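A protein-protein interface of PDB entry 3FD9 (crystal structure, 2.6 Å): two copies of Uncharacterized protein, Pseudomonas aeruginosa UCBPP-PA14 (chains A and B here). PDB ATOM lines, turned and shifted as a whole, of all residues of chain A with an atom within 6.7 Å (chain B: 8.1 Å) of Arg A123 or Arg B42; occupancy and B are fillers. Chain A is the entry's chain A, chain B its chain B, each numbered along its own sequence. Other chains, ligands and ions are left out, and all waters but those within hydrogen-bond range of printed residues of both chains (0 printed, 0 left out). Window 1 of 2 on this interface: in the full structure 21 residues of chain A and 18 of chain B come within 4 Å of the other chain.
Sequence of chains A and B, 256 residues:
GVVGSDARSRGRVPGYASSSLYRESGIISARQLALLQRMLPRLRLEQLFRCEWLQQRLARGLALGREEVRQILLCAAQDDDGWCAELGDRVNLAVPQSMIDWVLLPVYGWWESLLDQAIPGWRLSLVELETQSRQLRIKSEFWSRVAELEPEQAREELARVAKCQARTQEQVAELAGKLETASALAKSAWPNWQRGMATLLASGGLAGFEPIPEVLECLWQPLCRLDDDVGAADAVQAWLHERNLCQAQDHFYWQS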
ATOM      1  N   TYR A 108      -7.875  26.633  -1.268  1.00  0.00           N
ATOM      2  CA  TYR A 108      -6.759  25.698  -1.165  1.00  0.00           C
ATOM      3  C   TYR A 108      -6.885  24.830   0.069  1.00  0.00           C
ATOM      4  O   TYR A 108      -6.529  23.665   0.049  1.00  0.00           O
ATOM      5  CB  TYR A 108      -5.416  26.427  -1.147  1.00  0.00           C
ATOM      6  CG  TYR A 108      -4.249  25.474  -1.177  1.00  0.00           C
ATOM      7  CD1 TYR A 108      -3.608  25.163  -2.377  1.00  0.00           C
ATOM      8  CD2 TYR A 108      -3.802  24.859  -0.017  1.00  0.00           C
ATOM      9  CE1 TYR A 108      -2.540  24.279  -2.413  1.00  0.00           C
ATOM     10  CE2 TYR A 108      -2.743  23.975  -0.042  1.00  0.00           C
ATOM     11  CZ  TYR A 108      -2.116  23.689  -1.243  1.00  0.00           C
ATOM     12  OH  TYR A 108      -1.057  22.817  -1.264  1.00  0.00           O
ATOM     13  N   GLU A 112      -7.118  20.913  -0.370  1.00  0.00           N
ATOM     14  CA  GLU A 112      -6.279  20.107   0.499  1.00  0.00           C
ATOM     15  C   GLU A 112      -7.044  18.988   1.222  1.00  0.00           C
ATOM     16  O   GLU A 112      -6.547  17.868   1.336  1.00  0.00           O
ATOM     17  CB  GLU A 112      -5.631  21.027   1.523  1.00  0.00           C
ATOM     18  CG  GLU A 112      -4.434  20.461   2.209  1.00  0.00           C
ATOM     19  CD  GLU A 112      -3.939  21.385   3.284  1.00  0.00           C
ATOM     20  OE1 GLU A 112      -4.776  21.884   4.072  1.00  0.00           O
ATOM     21  OE2 GLU A 112      -2.715  21.621   3.333  1.00  0.00           O
ATOM     22  N   ALA A 118      -8.368  14.355   7.066  1.00  0.00           N
ATOM     23  CA  ALA A 118      -7.890  14.432   8.443  1.00  0.00           C
ATOM     24  C   ALA A 118      -6.983  15.636   8.656  1.00  0.00           C
ATOM     25  O   ALA A 118      -6.725  16.039   9.792  1.00  0.00           O
ATOM     26  CB  ALA A 118      -7.167  13.149   8.822  1.00  0.00           C
ATOM     27  N   ILE A 119      -6.511  16.201   7.549  1.00  0.00           N
ATOM     28  CA  ILE A 119      -5.562  17.309   7.562  1.00  0.00           C
ATOM     29  C   ILE A 119      -6.031  18.524   8.353  1.00  0.00           C
ATOM     30  O   ILE A 119      -5.315  18.999   9.234  1.00  0.00           O
ATOM     31  CB  ILE A 119      -5.206  17.762   6.140  1.00  0.00           C
ATOM     32  CG1 ILE A 119      -4.474  16.655   5.392  1.00  0.00           C
ATOM     33  CG2 ILE A 119      -4.337  19.013   6.185  1.00  0.00           C
ATOM     34  CD1 ILE A 119      -3.767  17.150   4.141  1.00  0.00           C
ATOM     35  N   PRO A 120      -7.225  19.051   8.034  1.00  0.00           N
ATOM     36  CA  PRO A 120      -7.673  20.231   8.782  1.00  0.00           C
ATOM     37  C   PRO A 120      -7.543  19.997  10.272  1.00  0.00           C
ATOM     38  O   PRO A 120      -7.056  20.869  10.985  1.00  0.00           O
ATOM     39  CB  PRO A 120      -9.144  20.343   8.408  1.00  0.00           C
ATOM     40  CG  PRO A 120      -9.232  19.704   7.069  1.00  0.00           C
ATOM     41  CD  PRO A 120      -8.232  18.597   7.062  1.00  0.00           C
ATOM     42  N   GLY A 121      -7.955  18.819  10.731  1.00  0.00           N
ATOM     43  CA  GLY A 121      -7.900  18.483  12.140  1.00  0.00           C
ATOM     44  C   GLY A 121      -6.486  18.494  12.688  1.00  0.00           C
ATOM     45  O   GLY A 121      -6.246  18.951  13.809  1.00  0.00           O
ATOM     46  N   TRP A 122      -5.543  17.990  11.899  1.00  0.00           N
ATOM     47  CA  TRP A 122      -4.150  17.984  12.325  1.00  0.00           C
ATOM     48  C   TRP A 122      -3.618  19.401  12.543  1.00  0.00           C
ATOM     49  O   TRP A 122      -2.932  19.666  13.534  1.00  0.00           O
ATOM     50  CB  TRP A 122      -3.266  17.252  11.312  1.00  0.00           C
ATOM     51  CG  TRP A 122      -3.666  15.833  11.072  1.00  0.00           C
ATOM     52  CD1 TRP A 122      -4.477  15.064  11.859  1.00  0.00           C
ATOM     53  CD2 TRP A 122      -3.252  14.995   9.985  1.00  0.00           C
ATOM     54  NE1 TRP A 122      -4.602  13.807  11.320  1.00  0.00           N
ATOM     55  CE2 TRP A 122      -3.858  13.737  10.170  1.00  0.00           C
ATOM     56  CE3 TRP A 122      -2.431  15.190   8.867  1.00  0.00           C
ATOM     57  CZ2 TRP A 122      -3.674  12.678   9.283  1.00  0.00           C
ATOM     58  CZ3 TRP A 122      -2.247  14.138   7.985  1.00  0.00           C
ATOM     59  CH2 TRP A 122      -2.866  12.896   8.199  1.00  0.00           C
ATOM     60  N   ARG A 123      -3.936  20.303  11.614  1.00  0.00           N
ATOM     61  CA  ARG A 123      -3.418  21.665  11.661  1.00  0.00           C
ATOM     62  C   ARG A 123      -3.790  22.374  12.945  1.00  0.00           C
ATOM     63  O   ARG A 123      -2.916  22.882  13.655  1.00  0.00           O
ATOM     64  CB  ARG A 123      -3.891  22.484  10.457  1.00  0.00           C
ATOM     65  CG  ARG A 123      -3.207  22.091   9.159  1.00  0.00           C
ATOM     66  CD  ARG A 123      -3.525  23.040   8.026  1.00  0.00           C
ATOM     67  NE  ARG A 123      -2.919  22.569   6.781  1.00  0.00           N
ATOM     68  CZ  ARG A 123      -1.606  22.460   6.582  1.00  0.00           C
ATOM     69  NH1 ARG A 123      -0.754  22.787   7.550  1.00  0.00           N
ATOM     70  NH2 ARG A 123      -1.140  22.021   5.418  1.00  0.00           N
ATOM     71  N   LEU A 124      -5.085  22.414  13.246  1.00  0.00           N
ATOM     72  CA  LEU A 124      -5.536  23.108  14.444  1.00  0.00           C
ATOM     73  C   LEU A 124      -5.014  22.410  15.693  1.00  0.00           C
ATOM     74  O   LEU A 124      -4.696  23.060  16.684  1.00  0.00           O
ATOM     75  CB  LEU A 124      -7.059  23.247  14.472  1.00  0.00           C
ATOM     76  CG  LEU A 124      -7.915  21.996  14.631  1.00  0.00           C
ATOM     77  CD1 LEU A 124      -8.086  21.653  16.103  1.00  0.00           C
ATOM     78  CD2 LEU A 124      -9.270  22.219  13.976  1.00  0.00           C
ATOM     79  N   SER A 125      -4.905  21.088  15.636  1.00  0.00           N
ATOM     80  CA  SER A 125      -4.328  20.345  16.749  1.00  0.00           C
ATOM     81  C   SER A 125      -2.924  20.852  17.050  1.00  0.00           C
ATOM     82  O   SER A 125      -2.526  20.945  18.211  1.00  0.00           O
ATOM     83  CB  SER A 125      -4.298  18.844  16.457  1.00  0.00           C
ATOM     84  OG  SER A 125      -5.609  18.308  16.396  1.00  0.00           O
ATOM     85  N   LEU A 126      -2.171  21.172  16.004  1.00  0.00           N
ATOM     86  CA  LEU A 126      -0.864  21.786  16.186  1.00  0.00           C
ATOM     87  C   LEU A 126      -1.012  23.092  16.947  1.00  0.00           C
ATOM     88  O   LEU A 126      -0.298  23.339  17.919  1.00  0.00           O
ATOM     89  CB  LEU A 126      -0.180  22.046  14.846  1.00  0.00           C
ATOM     90  CG  LEU A 126       0.792  20.963  14.383  1.00  0.00           C
ATOM     91  CD1 LEU A 126       1.639  21.472  13.227  1.00  0.00           C
ATOM     92  CD2 LEU A 126       1.670  20.514  15.542  1.00  0.00           C
ATOM     93  N   VAL A 127      -1.948  23.923  16.501  1.00  0.00           N
ATOM     94  CA  VAL A 127      -2.184  25.210  17.133  1.00  0.00           C
ATOM     95  C   VAL A 127      -2.387  25.036  18.631  1.00  0.00           C
ATOM     96  O   VAL A 127      -1.779  25.745  19.433  1.00  0.00           O
ATOM     97  CB  VAL A 127      -3.401  25.922  16.530  1.00  0.00           C
ATOM     98  CG1 VAL A 127      -3.705  27.196  17.308  1.00  0.00           C
ATOM     99  CG2 VAL A 127      -3.152  26.241  15.058  1.00  0.00           C
ATOM    100  N   GLU A 128      -3.232  24.083  19.008  1.00  0.00           N
ATOM    101  CA  GLU A 128      -3.507  23.838  20.418  1.00  0.00           C
ATOM    102  C   GLU A 128      -2.308  23.210  21.106  1.00  0.00           C
ATOM    103  O   GLU A 128      -2.115  23.363  22.313  1.00  0.00           O
ATOM    104  CB  GLU A 128      -4.738  22.949  20.577  1.00  0.00           C
ATOM    105  CG  GLU A 128      -6.025  23.632  20.162  1.00  0.00           C
ATOM    106  CD  GLU A 128      -7.209  22.684  20.142  1.00  0.00           C
ATOM    107  OE1 GLU A 128      -7.172  21.662  20.867  1.00  0.00           O
ATOM    108  OE2 GLU A 128      -8.178  22.964  19.401  1.00  0.00           O
ATOM    109  N   LEU A 175       2.404  14.812  14.354  1.00  0.00           N
ATOM    110  CA  LEU A 175       1.557  15.687  13.553  1.00  0.00           C
ATOM    111  C   LEU A 175       2.357  16.326  12.419  1.00  0.00           C
ATOM    112  O   LEU A 175       2.000  16.202  11.247  1.00  0.00           O
ATOM    113  CB  LEU A 175       0.930  16.774  14.423  1.00  0.00           C
ATOM    114  CG  LEU A 175      -0.381  16.458  15.146  1.00  0.00           C
ATOM    115  CD1 LEU A 175      -1.443  16.020  14.150  1.00  0.00           C
ATOM    116  CD2 LEU A 175      -0.181  15.399  16.216  1.00  0.00           C
ATOM    117  N   ALA A 176       3.441  17.007  12.770  1.00  0.00           N
ATOM    118  CA  ALA A 176       4.303  17.622  11.767  1.00  0.00           C
ATOM    119  C   ALA A 176       4.749  16.600  10.730  1.00  0.00           C
ATOM    120  O   ALA A 176       5.009  16.948   9.582  1.00  0.00           O
ATOM    121  CB  ALA A 176       5.508  18.270  12.425  1.00  0.00           C
ATOM    122  N   LEU A 179       1.768  15.817   8.323  1.00  0.00           N
ATOM    123  CA  LEU A 179       1.528  17.001   7.515  1.00  0.00           C
ATOM    124  C   LEU A 179       2.630  17.201   6.488  1.00  0.00           C
ATOM    125  O   LEU A 179       2.395  17.746   5.407  1.00  0.00           O
ATOM    126  CB  LEU A 179       1.413  18.238   8.404  1.00  0.00           C
ATOM    127  CG  LEU A 179       0.140  18.367   9.240  1.00  0.00           C
ATOM    128  CD1 LEU A 179       0.377  19.256  10.440  1.00  0.00           C
ATOM    129  CD2 LEU A 179      -1.004  18.905   8.402  1.00  0.00           C
ATOM    130  N   GLU A 180       3.841  16.773   6.821  1.00  0.00           N
ATOM    131  CA  GLU A 180       4.948  16.902   5.889  1.00  0.00           C
ATOM    132  C   GLU A 180       4.702  15.954   4.728  1.00  0.00           C
ATOM    133  O   GLU A 180       4.917  16.299   3.571  1.00  0.00           O
ATOM    134  CB  GLU A 180       6.279  16.586   6.568  1.00  0.00           C
ATOM    135  CG  GLU A 180       7.430  17.477   6.114  1.00  0.00           C
ATOM    136  CD  GLU A 180       7.691  17.393   4.620  1.00  0.00           C
ATOM    137  OE1 GLU A 180       7.987  16.282   4.126  1.00  0.00           O
ATOM    138  OE2 GLU A 180       7.613  18.441   3.942  1.00  0.00           O
ATOM    139  N   ALA A 182       1.686  14.758   3.739  1.00  0.00           N
ATOM    140  CA  ALA A 182       0.548  15.265   2.978  1.00  0.00           C
ATOM    141  C   ALA A 182       0.987  16.385   2.047  1.00  0.00           C
ATOM    142  O   ALA A 182       0.638  16.406   0.866  1.00  0.00           O
ATOM    143  CB  ALA A 182      -0.544  15.749   3.906  1.00  0.00           C
ATOM    144  N   SER A 183       1.764  17.315   2.589  1.00  0.00           N
ATOM    145  CA  SER A 183       2.303  18.412   1.800  1.00  0.00           C
ATOM    146  C   SER A 183       2.934  17.908   0.505  1.00  0.00           C
ATOM    147  O   SER A 183       2.700  18.463  -0.563  1.00  0.00           O
ATOM    148  CB  SER A 183       3.325  19.205   2.619  1.00  0.00           C
ATOM    149  OG  SER A 183       4.143  20.010   1.783  1.00  0.00           O
ATOM    150  N   SER B  19       5.684  31.709  16.311  1.00  0.00           N
ATOM    151  CA  SER B  19       4.597  32.484  15.742  1.00  0.00           C
ATOM    152  C   SER B  19       4.061  33.461  16.771  1.00  0.00           C
ATOM    153  O   SER B  19       4.061  34.671  16.554  1.00  0.00           O
ATOM    154  CB  SER B  19       3.459  31.567  15.298  1.00  0.00           C
ATOM    155  OG  SER B  19       3.945  30.427  14.611  1.00  0.00           O
ATOM    156  N   LEU B  33       0.307  35.918   8.900  1.00  0.00           N
ATOM    157  CA  LEU B  33       0.807  34.629   9.351  1.00  0.00           C
ATOM    158  C   LEU B  33       0.101  33.529   8.582  1.00  0.00           C
ATOM    159  O   LEU B  33       0.713  32.528   8.233  1.00  0.00           O
ATOM    160  CB  LEU B  33       0.609  34.441  10.855  1.00  0.00           C
ATOM    161  CG  LEU B  33       1.072  33.089  11.416  1.00  0.00           C
ATOM    162  CD1 LEU B  33       2.576  32.925  11.332  1.00  0.00           C
ATOM    163  CD2 LEU B  33       0.626  32.925  12.862  1.00  0.00           C
ATOM    164  N   LEU B  36       1.716  33.227   5.174  1.00  0.00           N
ATOM    165  CA  LEU B  36       3.067  32.702   5.356  1.00  0.00           C
ATOM    166  C   LEU B  36       3.024  31.224   5.662  1.00  0.00           C
ATOM    167  O   LEU B  36       3.804  30.444   5.122  1.00  0.00           O
ATOM    168  CB  LEU B  36       3.788  33.426   6.492  1.00  0.00           C
ATOM    169  CG  LEU B  36       4.299  34.820   6.129  1.00  0.00           C
ATOM    170  CD1 LEU B  36       5.042  35.457   7.289  1.00  0.00           C
ATOM    171  CD2 LEU B  36       5.201  34.734   4.896  1.00  0.00           C
ATOM    172  N   GLN B  37       2.101  30.849   6.539  1.00  0.00           N
ATOM    173  CA  GLN B  37       2.017  29.491   7.046  1.00  0.00           C
ATOM    174  C   GLN B  37       1.665  28.534   5.917  1.00  0.00           C
ATOM    175  O   GLN B  37       2.123  27.394   5.883  1.00  0.00           O
ATOM    176  CB  GLN B  37       0.952  29.428   8.129  1.00  0.00           C
ATOM    177  CG  GLN B  37       1.418  28.788   9.413  1.00  0.00           C
ATOM    178  CD  GLN B  37       0.606  29.256  10.603  1.00  0.00           C
ATOM    179  OE1 GLN B  37      -0.588  29.546  10.480  1.00  0.00           O
ATOM    180  NE2 GLN B  37       1.251  29.342  11.762  1.00  0.00           N
ATOM    181  N   ARG B  38       0.857  29.021   4.985  1.00  0.00           N
ATOM    182  CA  ARG B  38       0.388  28.221   3.863  1.00  0.00           C
ATOM    183  C   ARG B  38       1.405  28.157   2.726  1.00  0.00           C
ATOM    184  O   ARG B  38       1.440  27.183   1.977  1.00  0.00           O
ATOM    185  CB  ARG B  38      -0.940  28.778   3.345  1.00  0.00           C
ATOM    186  CG  ARG B  38      -1.364  28.199   2.020  1.00  0.00           C
ATOM    187  CD  ARG B  38      -1.605  26.705   2.129  1.00  0.00           C
ATOM    188  NE  ARG B  38      -2.884  26.400   2.766  1.00  0.00           N
ATOM    189  CZ  ARG B  38      -3.140  25.270   3.418  1.00  0.00           C
ATOM    190  NH1 ARG B  38      -2.199  24.339   3.530  1.00  0.00           N
ATOM    191  NH2 ARG B  38      -4.331  25.075   3.972  1.00  0.00           N
ATOM    192  N   MET B  39       2.223  29.196   2.587  1.00  0.00           N
ATOM    193  CA  MET B  39       3.186  29.254   1.488  1.00  0.00           C
ATOM    194  C   MET B  39       4.535  28.632   1.839  1.00  0.00           C
ATOM    195  O   MET B  39       5.173  28.016   0.992  1.00  0.00           O
ATOM    196  CB  MET B  39       3.381  30.689   1.000  1.00  0.00           C
ATOM    197  CG  MET B  39       2.136  31.297   0.403  1.00  0.00           C
ATOM    198  SD  MET B  39       1.264  30.182  -0.972  1.00  0.00           S
ATOM    199  CE  MET B  39      -0.540  30.861  -0.740  1.00  0.00           C
ATOM    200  N   LEU B  40       4.968  28.797   3.084  1.00  0.00           N
ATOM    201  CA  LEU B  40       6.246  28.256   3.523  1.00  0.00           C
ATOM    202  C   LEU B  40       6.090  26.923   4.251  1.00  0.00           C
ATOM    203  O   LEU B  40       5.305  26.805   5.196  1.00  0.00           O
ATOM    204  CB  LEU B  40       6.950  29.247   4.448  1.00  0.00           C
ATOM    205  CG  LEU B  40       7.254  30.645   3.915  1.00  0.00           C
ATOM    206  CD1 LEU B  40       8.065  31.419   4.933  1.00  0.00           C
ATOM    207  CD2 LEU B  40       7.995  30.560   2.601  1.00  0.00           C
ATOM    208  N   PRO B  41       6.843  25.906   3.815  1.00  0.00           N
ATOM    209  CA  PRO B  41       6.897  24.623   4.524  1.00  0.00           C
ATOM    210  C   PRO B  41       7.354  24.838   5.961  1.00  0.00           C
ATOM    211  O   PRO B  41       8.062  25.811   6.213  1.00  0.00           O
ATOM    212  CB  PRO B  41       7.969  23.850   3.757  1.00  0.00           C
ATOM    213  CG  PRO B  41       7.988  24.468   2.397  1.00  0.00           C
ATOM    214  CD  PRO B  41       7.654  25.909   2.586  1.00  0.00           C
ATOM    215  N   ARG B  42       6.973  23.951   6.878  1.00  0.00           N
ATOM    216  CA  ARG B  42       7.333  24.105   8.288  1.00  0.00           C
ATOM    217  C   ARG B  42       8.813  24.424   8.480  1.00  0.00           C
ATOM    218  O   ARG B  42       9.178  25.197   9.360  1.00  0.00           O
ATOM    219  CB  ARG B  42       6.982  22.849   9.088  1.00  0.00           C
ATOM    220  CG  ARG B  42       5.507  22.483   9.092  1.00  0.00           C
ATOM    221  CD  ARG B  42       4.629  23.638   9.572  1.00  0.00           C
ATOM    222  NE  ARG B  42       3.216  23.259   9.646  1.00  0.00           N
ATOM    223  CZ  ARG B  42       2.221  24.107   9.895  1.00  0.00           C
ATOM    224  NH1 ARG B  42       2.481  25.395  10.094  1.00  0.00           N
ATOM    225  NH2 ARG B  42       0.968  23.667   9.943  1.00  0.00           N
ATOM    226  N   LEU B  43       9.661  23.821   7.654  1.00  0.00           N
ATOM    227  CA  LEU B  43      11.108  23.958   7.794  1.00  0.00           C
ATOM    228  C   LEU B  43      11.586  25.364   7.454  1.00  0.00           C
ATOM    229  O   LEU B  43      12.476  25.902   8.119  1.00  0.00           O
ATOM    230  CB  LEU B  43      11.830  22.916   6.931  1.00  0.00           C
ATOM    231  CG  LEU B  43      13.351  23.026   6.771  1.00  0.00           C
ATOM    232  CD1 LEU B  43      14.053  23.165   8.123  1.00  0.00           C
ATOM    233  CD2 LEU B  43      13.901  21.833   5.985  1.00  0.00           C
ATOM    234  N   ARG B  44      10.998  25.951   6.415  1.00  0.00           N
ATOM    235  CA  ARG B  44      11.367  27.299   5.993  1.00  0.00           C
ATOM    236  C   ARG B  44      10.795  28.298   6.979  1.00  0.00           C
ATOM    237  O   ARG B  44      11.428  29.298   7.315  1.00  0.00           O
ATOM    238  CB  ARG B  44      10.839  27.612   4.592  1.00  0.00           C
ATOM    239  CG  ARG B  44      10.902  26.461   3.609  1.00  0.00           C
ATOM    240  CD  ARG B  44      12.281  25.829   3.547  1.00  0.00           C
ATOM    241  NE  ARG B  44      13.241  26.647   2.818  1.00  0.00           N
ATOM    242  CZ  ARG B  44      14.495  26.277   2.575  1.00  0.00           C
ATOM    243  NH1 ARG B  44      14.937  25.101   3.006  1.00  0.00           N
ATOM    244  NH2 ARG B  44      15.304  27.081   1.899  1.00  0.00           N
ATOM    245  N   LEU B  45       9.579  28.017   7.432  1.00  0.00           N
ATOM    246  CA  LEU B  45       8.891  28.873   8.378  1.00  0.00           C
ATOM    247  C   LEU B  45       9.742  28.996   9.626  1.00  0.00           C
ATOM    248  O   LEU B  45      10.007  30.094  10.095  1.00  0.00           O
ATOM    249  CB  LEU B  45       7.534  28.277   8.734  1.00  0.00           C
ATOM    250  CG  LEU B  45       6.302  29.172   8.622  1.00  0.00           C
ATOM    251  CD1 LEU B  45       5.287  28.758   9.674  1.00  0.00           C
ATOM    252  CD2 LEU B  45       6.674  30.631   8.795  1.00  0.00           C
ATOM    253  N   GLU B  46      10.189  27.869  10.159  1.00  0.00           N
ATOM    254  CA  GLU B  46      11.019  27.900  11.351  1.00  0.00           C
ATOM    255  C   GLU B  46      12.296  28.697  11.117  1.00  0.00           C
ATOM    256  O   GLU B  46      12.696  29.483  11.972  1.00  0.00           O
ATOM    257  CB  GLU B  46      11.335  26.489  11.850  1.00  0.00           C
ATOM    258  CG  GLU B  46      10.131  25.760  12.461  1.00  0.00           C
ATOM    259  CD  GLU B  46       9.319  26.640  13.423  1.00  0.00           C
ATOM    260  OE1 GLU B  46       9.926  27.489  14.121  1.00  0.00           O
ATOM    261  OE2 GLU B  46       8.074  26.478  13.487  1.00  0.00           O
ATOM    262  N   GLN B  47      12.925  28.502   9.960  1.00  0.00           N
ATOM    263  CA  GLN B  47      14.130  29.256   9.603  1.00  0.00           C
ATOM    264  C   GLN B  47      13.827  30.744   9.581  1.00  0.00           C
ATOM    265  O   GLN B  47      14.603  31.545  10.089  1.00  0.00           O
ATOM    266  CB  GLN B  47      14.685  28.815   8.244  1.00  0.00           C
ATOM    267  CG  GLN B  47      15.372  27.453   8.255  1.00  0.00           C
ATOM    268  CD  GLN B  47      15.630  26.889   6.860  1.00  0.00           C
ATOM    269  OE1 GLN B  47      15.063  27.347   5.866  1.00  0.00           O
ATOM    270  NE2 GLN B  47      16.489  25.880   6.789  1.00  0.00           N
ATOM    271  N   LEU B  48      12.689  31.107   8.997  1.00  0.00           N
ATOM    272  CA  LEU B  48      12.249  32.496   8.977  1.00  0.00           C
ATOM    273  C   LEU B  48      12.294  33.086  10.382  1.00  0.00           C
ATOM    274  O   LEU B  48      13.033  34.037  10.650  1.00  0.00           O
ATOM    275  CB  LEU B  48      10.830  32.600   8.425  1.00  0.00           C
ATOM    276  CG  LEU B  48      10.304  34.031   8.295  1.00  0.00           C
ATOM    277  CD1 LEU B  48      11.061  34.768   7.219  1.00  0.00           C
ATOM    278  CD2 LEU B  48       8.820  34.056   7.995  1.00  0.00           C
ATOM    279  N   PHE B  49      11.512  32.497  11.280  1.00  0.00           N
ATOM    280  CA  PHE B  49      11.392  32.985  12.648  1.00  0.00           C
ATOM    281  C   PHE B  49      12.726  33.108  13.390  1.00  0.00           C
ATOM    282  O   PHE B  49      12.888  33.984  14.233  1.00  0.00           O
ATOM    283  CB  PHE B  49      10.422  32.103  13.439  1.00  0.00           C
ATOM    284  CG  PHE B  49       9.010  32.127  12.909  1.00  0.00           C
ATOM    285  CD1 PHE B  49       8.527  33.235  12.234  1.00  0.00           C
ATOM    286  CD2 PHE B  49       8.163  31.052  13.104  1.00  0.00           C
ATOM    287  CE1 PHE B  49       7.237  33.271  11.754  1.00  0.00           C
ATOM    288  CE2 PHE B  49       6.857  31.076  12.624  1.00  0.00           C
ATOM    289  CZ  PHE B  49       6.395  32.190  11.951  1.00  0.00           C
ATOM    290  N   ARG B  50      13.683  32.240  13.081  1.00  0.00           N
ATOM    291  CA  ARG B  50      14.982  32.285  13.746  1.00  0.00           C
ATOM    292  C   ARG B  50      15.970  33.219  13.056  1.00  0.00           C
ATOM    293  O   ARG B  50      17.018  33.536  13.612  1.00  0.00           O
ATOM    294  CB  ARG B  50      15.616  30.897  13.793  1.00  0.00           C
ATOM    295  CG  ARG B  50      14.758  29.795  14.381  1.00  0.00           C
ATOM    296  CD  ARG B  50      15.603  28.538  14.568  1.00  0.00           C
ATOM    297  NE  ARG B  50      16.653  28.437  13.548  1.00  0.00           N
ATOM    298  CZ  ARG B  50      16.606  27.630  12.488  1.00  0.00           C
ATOM    299  NH1 ARG B  50      15.562  26.829  12.298  1.00  0.00           N
ATOM    300  NH2 ARG B  50      17.612  27.618  11.620  1.00  0.00           N
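NH2 of Arg A123 lies close to NH1 of Arg B38.
The side-chain carboxylate (OE2) of Glu A112 lies within salt-bridge range of the guanidinium group (NH1) of Arg B38 (2.8 Å).
The guanidinium group (NH1) of Arg A123 sits close to the guanidinium group (NH2) of Arg B42, at 3.1 Å.
CD2 of Tyr A108 touches NE of Arg B38 (3.3 Å).
No position is printed for both chains.
Of the 4 pairs that touch across the chains among the printed residues, none has its exchanged pair printed and touching as well.
The side-chain carboxylate of Glu A112 is in salt-bridge range of the guanidinium group of Arg A123, 2.6 Å away.
Printed residues of chain B that touch a printed residue of chain A: Arg B38 and Arg B42.
Among the printed residues, Asp or Glu carboxylates within 4 Å of a Lys or Arg side-chain nitrogen of the other chain: Glu A112 with Arg B38.
Of chain B, only Arg B38 and Arg B42 come within 4 Å of Arg A123.
Of the printed residues of chain B, Tyr A108 touches Arg B38.
Of the printed residues of chain B, Glu A112 touches Arg B38.
Of the printed residues of chain A, Arg B38 touches Tyr A108, Glu A112 and Arg A123.
Glu B46 touches none of the printed residues of chain A.
The nearest residue of chain B that does not touch Arg A123 is Gln B37 (5.7 Å).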
